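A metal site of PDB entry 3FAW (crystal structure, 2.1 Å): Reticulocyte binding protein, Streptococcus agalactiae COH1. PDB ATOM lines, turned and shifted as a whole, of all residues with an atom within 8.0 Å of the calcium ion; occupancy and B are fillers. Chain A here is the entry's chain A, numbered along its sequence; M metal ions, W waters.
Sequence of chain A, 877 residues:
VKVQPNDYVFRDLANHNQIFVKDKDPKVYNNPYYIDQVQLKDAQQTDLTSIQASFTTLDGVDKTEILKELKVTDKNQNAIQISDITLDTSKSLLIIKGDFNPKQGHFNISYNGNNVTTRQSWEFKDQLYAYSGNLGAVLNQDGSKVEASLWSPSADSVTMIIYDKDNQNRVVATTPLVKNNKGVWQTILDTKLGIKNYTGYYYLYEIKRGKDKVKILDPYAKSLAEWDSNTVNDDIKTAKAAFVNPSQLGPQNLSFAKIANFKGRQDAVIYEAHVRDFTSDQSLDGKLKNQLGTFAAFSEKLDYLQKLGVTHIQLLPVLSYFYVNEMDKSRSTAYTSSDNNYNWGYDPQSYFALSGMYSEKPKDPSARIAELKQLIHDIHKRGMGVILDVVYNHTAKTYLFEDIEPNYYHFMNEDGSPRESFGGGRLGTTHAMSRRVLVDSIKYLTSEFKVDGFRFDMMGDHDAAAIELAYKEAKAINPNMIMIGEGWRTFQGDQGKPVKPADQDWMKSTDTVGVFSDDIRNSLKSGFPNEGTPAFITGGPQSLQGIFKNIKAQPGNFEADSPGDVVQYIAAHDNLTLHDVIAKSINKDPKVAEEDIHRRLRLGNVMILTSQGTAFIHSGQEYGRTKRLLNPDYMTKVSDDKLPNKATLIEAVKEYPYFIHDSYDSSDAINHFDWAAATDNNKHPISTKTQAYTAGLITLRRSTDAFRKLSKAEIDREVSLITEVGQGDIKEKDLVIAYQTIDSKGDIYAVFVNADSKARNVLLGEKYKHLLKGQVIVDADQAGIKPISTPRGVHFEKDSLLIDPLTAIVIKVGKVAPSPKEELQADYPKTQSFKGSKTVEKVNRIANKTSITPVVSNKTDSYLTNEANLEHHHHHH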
ATOM      1  N   ARG A 265      21.192  18.146 -10.072  1.00  0.00           N
ATOM      2  CA  ARG A 265      19.728  18.100  -9.998  1.00  0.00           C
ATOM      3  C   ARG A 265      19.160  16.697  -9.706  1.00  0.00           C
ATOM      4  O   ARG A 265      18.098  16.560  -9.106  1.00  0.00           O
ATOM      5  CB  ARG A 265      19.104  18.700 -11.273  1.00  0.00           C
ATOM      6  CG  ARG A 265      19.555  18.059 -12.574  1.00  0.00           C
ATOM      7  CD  ARG A 265      19.133  18.877 -13.788  1.00  0.00           C
ATOM      8  NE  ARG A 265      19.539  18.221 -15.036  1.00  0.00           N
ATOM      9  CZ  ARG A 265      18.972  18.394 -16.230  1.00  0.00           C
ATOM     10  NH1 ARG A 265      17.944  19.232 -16.377  1.00  0.00           N
ATOM     11  NH2 ARG A 265      19.424  17.721 -17.284  1.00  0.00           N
ATOM     12  N   GLN A 504       7.942  19.979 -22.463  1.00  0.00           N
ATOM     13  CA  GLN A 504       8.555  18.641 -22.403  1.00  0.00           C
ATOM     14  C   GLN A 504       9.402  18.281 -23.629  1.00  0.00           C
ATOM     15  O   GLN A 504      10.358  17.520 -23.508  1.00  0.00           O
ATOM     16  CB  GLN A 504       7.469  17.576 -22.184  1.00  0.00           C
ATOM     17  CG  GLN A 504       7.052  17.408 -20.730  1.00  0.00           C
ATOM     18  CD  GLN A 504       5.871  16.452 -20.552  1.00  0.00           C
ATOM     19  OE1 GLN A 504       5.101  16.213 -21.475  1.00  0.00           O
ATOM     20  NE2 GLN A 504       5.731  15.914 -19.336  1.00  0.00           N
ATOM     21  N   TRP A 506      11.287  20.374 -25.179  1.00  0.00           N
ATOM     22  CA  TRP A 506      12.525  21.141 -25.001  1.00  0.00           C
ATOM     23  C   TRP A 506      13.637  20.312 -24.322  1.00  0.00           C
ATOM     24  O   TRP A 506      14.818  20.635 -24.448  1.00  0.00           O
ATOM     25  CB  TRP A 506      12.226  22.394 -24.176  1.00  0.00           C
ATOM     26  CG  TRP A 506      13.373  23.295 -23.850  1.00  0.00           C
ATOM     27  CD1 TRP A 506      14.435  23.610 -24.654  1.00  0.00           C
ATOM     28  CD2 TRP A 506      13.554  24.040 -22.649  1.00  0.00           C
ATOM     29  NE1 TRP A 506      15.276  24.479 -24.012  1.00  0.00           N
ATOM     30  CE2 TRP A 506      14.755  24.768 -22.781  1.00  0.00           C
ATOM     31  CE3 TRP A 506      12.819  24.159 -21.458  1.00  0.00           C
ATOM     32  CZ2 TRP A 506      15.232  25.599 -21.767  1.00  0.00           C
ATOM     33  CZ3 TRP A 506      13.295  24.983 -20.459  1.00  0.00           C
ATOM     34  CH2 TRP A 506      14.494  25.694 -20.621  1.00  0.00           C
ATOM     35  N   MET A 507      13.241  19.244 -23.627  1.00  0.00           N
ATOM     36  CA  MET A 507      14.192  18.447 -22.845  1.00  0.00           C
ATOM     37  C   MET A 507      15.267  17.768 -23.690  1.00  0.00           C
ATOM     38  O   MET A 507      16.385  17.563 -23.229  1.00  0.00           O
ATOM     39  CB  MET A 507      13.456  17.408 -21.987  1.00  0.00           C
ATOM     40  CG  MET A 507      12.574  17.985 -20.872  1.00  0.00           C
ATOM     41  SD  MET A 507      13.420  19.055 -19.680  1.00  0.00           S
ATOM     42  CE  MET A 507      13.232  20.642 -20.511  1.00  0.00           C
ATOM     43  N   LYS A 508      14.955  17.437 -24.945  1.00  0.00           N
ATOM     44  CA  LYS A 508      15.947  16.829 -25.852  1.00  0.00           C
ATOM     45  C   LYS A 508      17.011  17.804 -26.375  1.00  0.00           C
ATOM     46  O   LYS A 508      17.967  17.353 -27.007  1.00  0.00           O
ATOM     47  CB  LYS A 508      15.251  16.138 -27.036  1.00  0.00           C
ATOM     48  CG  LYS A 508      14.656  17.088 -28.066  1.00  0.00           C
ATOM     49  CD  LYS A 508      13.850  16.331 -29.112  1.00  0.00           C
ATOM     50  CE  LYS A 508      13.148  17.286 -30.075  1.00  0.00           C
ATOM     51  NZ  LYS A 508      14.114  18.178 -30.794  1.00  0.00           N
ATOM     52  N   SER A 509      16.859  19.108 -26.130  1.00  0.00           N
ATOM     53  CA  SER A 509      17.769  20.135 -26.632  1.00  0.00           C
ATOM     54  C   SER A 509      18.349  21.020 -25.513  1.00  0.00           C
ATOM     55  O   SER A 509      18.919  22.078 -25.788  1.00  0.00           O
ATOM     56  CB  SER A 509      17.047  21.036 -27.644  1.00  0.00           C
ATOM     57  OG  SER A 509      16.482  20.273 -28.698  1.00  0.00           O
ATOM     58  N   THR A 510      18.207  20.588 -24.262  1.00  0.00           N
ATOM     59  CA  THR A 510      18.751  21.331 -23.123  1.00  0.00           C
ATOM     60  C   THR A 510      18.962  20.393 -21.942  1.00  0.00           C
ATOM     61  O   THR A 510      18.235  19.415 -21.779  1.00  0.00           O
ATOM     62  CB  THR A 510      17.803  22.505 -22.695  1.00  0.00           C
ATOM     63  OG1 THR A 510      18.444  23.301 -21.679  1.00  0.00           O
ATOM     64  CG2 THR A 510      16.493  21.970 -22.163  1.00  0.00           C
ATOM     65  N   ASP A 511      19.979  20.680 -21.134  1.00  0.00           N
ATOM     66  CA  ASP A 511      20.171  20.020 -19.836  1.00  0.00           C
ATOM     67  C   ASP A 511      20.234  21.095 -18.738  1.00  0.00           C
ATOM     68  O   ASP A 511      21.212  21.181 -17.998  1.00  0.00           O
ATOM     69  CB  ASP A 511      21.450  19.170 -19.806  1.00  0.00           C
ATOM     70  CG  ASP A 511      21.343  17.901 -20.646  1.00  0.00           C
ATOM     71  OD1 ASP A 511      20.240  17.493 -21.053  1.00  0.00           O
ATOM     72  OD2 ASP A 511      22.410  17.275 -20.889  1.00  0.00           O
ATOM     73  N   THR A 512      19.177  21.903 -18.651  1.00  0.00           N
ATOM     74  CA  THR A 512      19.109  22.998 -17.675  1.00  0.00           C
ATOM     75  C   THR A 512      17.937  22.786 -16.704  1.00  0.00           C
ATOM     76  O   THR A 512      18.144  22.466 -15.541  1.00  0.00           O
ATOM     77  CB  THR A 512      18.963  24.368 -18.389  1.00  0.00           C
ATOM     78  OG1 THR A 512      17.812  24.353 -19.241  1.00  0.00           O
ATOM     79  CG2 THR A 512      20.206  24.661 -19.226  1.00  0.00           C
ATOM     80  N   VAL A 513      16.716  22.959 -17.203  1.00  0.00           N
ATOM     81  CA  VAL A 513      15.511  22.857 -16.378  1.00  0.00           C
ATOM     82  C   VAL A 513      14.842  21.493 -16.587  1.00  0.00           C
ATOM     83  O   VAL A 513      14.701  21.040 -17.724  1.00  0.00           O
ATOM     84  CB  VAL A 513      14.520  23.983 -16.727  1.00  0.00           C
ATOM     85  CG1 VAL A 513      13.275  23.878 -15.871  1.00  0.00           C
ATOM     86  CG2 VAL A 513      15.185  25.343 -16.562  1.00  0.00           C
ATOM     87  N   PHE A 558       7.641  11.975 -23.757  1.00  0.00           N
ATOM     88  CA  PHE A 558       8.641  12.920 -24.271  1.00  0.00           C
ATOM     89  C   PHE A 558      10.037  12.311 -24.183  1.00  0.00           C
ATOM     90  O   PHE A 558      10.278  11.421 -23.378  1.00  0.00           O
ATOM     91  CB  PHE A 558       8.582  14.282 -23.561  1.00  0.00           C
ATOM     92  CG  PHE A 558       9.150  14.303 -22.162  1.00  0.00           C
ATOM     93  CD1 PHE A 558      10.517  14.536 -21.944  1.00  0.00           C
ATOM     94  CD2 PHE A 558       8.326  14.162 -21.047  1.00  0.00           C
ATOM     95  CE1 PHE A 558      11.033  14.573 -20.653  1.00  0.00           C
ATOM     96  CE2 PHE A 558       8.843  14.209 -19.755  1.00  0.00           C
ATOM     97  CZ  PHE A 558      10.200  14.415 -19.562  1.00  0.00           C
ATOM     98  N   GLU A 559      10.948  12.807 -25.028  1.00  0.00           N
ATOM     99  CA  GLU A 559      12.322  12.325 -25.050  1.00  0.00           C
ATOM    100  C   GLU A 559      13.177  13.018 -23.995  1.00  0.00           C
ATOM    101  O   GLU A 559      13.439  14.224 -24.094  1.00  0.00           O
ATOM    102  CB  GLU A 559      12.944  12.529 -26.446  1.00  0.00           C
ATOM    103  CG  GLU A 559      14.359  11.964 -26.626  1.00  0.00           C
ATOM    104  CD  GLU A 559      14.448  10.453 -26.434  1.00  0.00           C
ATOM    105  OE1 GLU A 559      13.440   9.759 -26.674  1.00  0.00           O
ATOM    106  OE2 GLU A 559      15.525   9.967 -26.051  1.00  0.00           O
ATOM    107  N   ALA A 560      13.603  12.259 -22.996  1.00  0.00           N
ATOM    108  CA  ALA A 560      14.582  12.747 -22.015  1.00  0.00           C
ATOM    109  C   ALA A 560      15.942  12.119 -22.313  1.00  0.00           C
ATOM    110  O   ALA A 560      16.149  10.930 -22.068  1.00  0.00           O
ATOM    111  CB  ALA A 560      14.128  12.385 -20.612  1.00  0.00           C
ATOM    112  N   ASP A 561      16.875  12.905 -22.835  1.00  0.00           N
ATOM    113  CA  ASP A 561      18.213  12.393 -23.166  1.00  0.00           C
ATOM    114  C   ASP A 561      19.162  12.386 -21.948  1.00  0.00           C
ATOM    115  O   ASP A 561      20.308  11.943 -22.066  1.00  0.00           O
ATOM    116  CB  ASP A 561      18.827  13.137 -24.367  1.00  0.00           C
ATOM    117  CG  ASP A 561      19.280  14.554 -24.046  1.00  0.00           C
ATOM    118  OD1 ASP A 561      18.628  15.235 -23.238  1.00  0.00           O
ATOM    119  OD2 ASP A 561      20.293  14.993 -24.629  1.00  0.00           O
ATOM    120  N   SER A 562      18.671  12.847 -20.804  1.00  0.00           N
ATOM    121  CA  SER A 562      19.412  12.831 -19.540  1.00  0.00           C
ATOM    122  C   SER A 562      18.413  12.639 -18.381  1.00  0.00           C
ATOM    123  O   SER A 562      17.302  13.176 -18.447  1.00  0.00           O
ATOM    124  CB  SER A 562      20.203  14.137 -19.379  1.00  0.00           C
ATOM    125  OG  SER A 562      20.627  14.343 -18.042  1.00  0.00           O
ATOM    126  N   PRO A 563      18.800  11.885 -17.335  1.00  0.00           N
ATOM    127  CA  PRO A 563      17.861  11.647 -16.223  1.00  0.00           C
ATOM    128  C   PRO A 563      17.441  12.913 -15.472  1.00  0.00           C
ATOM    129  O   PRO A 563      16.325  12.960 -14.951  1.00  0.00           O
ATOM    130  CB  PRO A 563      18.638  10.695 -15.302  1.00  0.00           C
ATOM    131  CG  PRO A 563      20.069  10.853 -15.680  1.00  0.00           C
ATOM    132  CD  PRO A 563      20.093  11.211 -17.117  1.00  0.00           C
ATOM    133  N   GLY A 564      18.315  13.912 -15.445  1.00  0.00           N
ATOM    134  CA  GLY A 564      18.011  15.203 -14.830  1.00  0.00           C
ATOM    135  C   GLY A 564      16.906  16.011 -15.505  1.00  0.00           C
ATOM    136  O   GLY A 564      16.388  16.970 -14.923  1.00  0.00           O
ATOM    137  N   ASP A 565      16.532  15.627 -16.726  1.00  0.00           N
ATOM    138  CA  ASP A 565      15.399  16.239 -17.432  1.00  0.00           C
ATOM    139  C   ASP A 565      14.046  15.912 -16.782  1.00  0.00           C
ATOM    140  O   ASP A 565      13.052  16.586 -17.076  1.00  0.00           O
ATOM    141  CB  ASP A 565      15.314  15.744 -18.879  1.00  0.00           C
ATOM    142  CG  ASP A 565      16.495  16.141 -19.719  1.00  0.00           C
ATOM    143  OD1 ASP A 565      17.199  17.123 -19.364  1.00  0.00           O
ATOM    144  OD2 ASP A 565      16.729  15.493 -20.758  1.00  0.00           O
ATOM    145  N   VAL A 566      14.019  14.885 -15.943  1.00  0.00           N
ATOM    146  CA  VAL A 566      12.775  14.304 -15.451  1.00  0.00           C
ATOM    147  C   VAL A 566      12.575  14.538 -13.956  1.00  0.00           C
ATOM    148  O   VAL A 566      13.431  14.183 -13.141  1.00  0.00           O
ATOM    149  CB  VAL A 566      12.766  12.784 -15.711  1.00  0.00           C
ATOM    150  CG1 VAL A 566      11.446  12.170 -15.260  1.00  0.00           C
ATOM    151  CG2 VAL A 566      13.002  12.495 -17.181  1.00  0.00           C
HETATM  152 CA    CA M   1      18.133  17.070 -21.954  1.00  0.00          CA
HETATM  153  O   HOH W   1      19.451  17.771 -23.839  1.00  0.00           O
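The side-chain carboxylate of Asp 511 sits close to the guanidinium group of Arg 265, at 3.9 Å.
OG1 of Thr 512 sits at hydrogen-bond distance from OG1 of Thr 510, at 2.7 Å.
The backbone NH (N) of Ser 562 lies close to the side-chain carboxylate (OD2) of Asp 565 (3.3 Å).
OD1 of Asp 565 lies close to NH2 of Arg 265 (3.1 Å).
Water W1 lies within hydrogen-bond range of OD2 of Asp 561 (3.0 Å) and N of Thr 510 (3.1 Å).
Of the 19 residues printed, 5 come within 4 Å of the calcium ion.
Along chain A the residues within 4 Å of the calcium ion span positions 507 to 565.
The calcium ion is bound by O of Met 507 (2.2 Å), OD1 of Asp 561 (2.3 Å), OD1 of Asp 511 (2.3 Å), O of Thr 510 (2.4 Å), water W1 (2.4 Å), OD2 of Asp 565 (2.4 Å) and OD1 of Asp 565 (2.8 Å).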
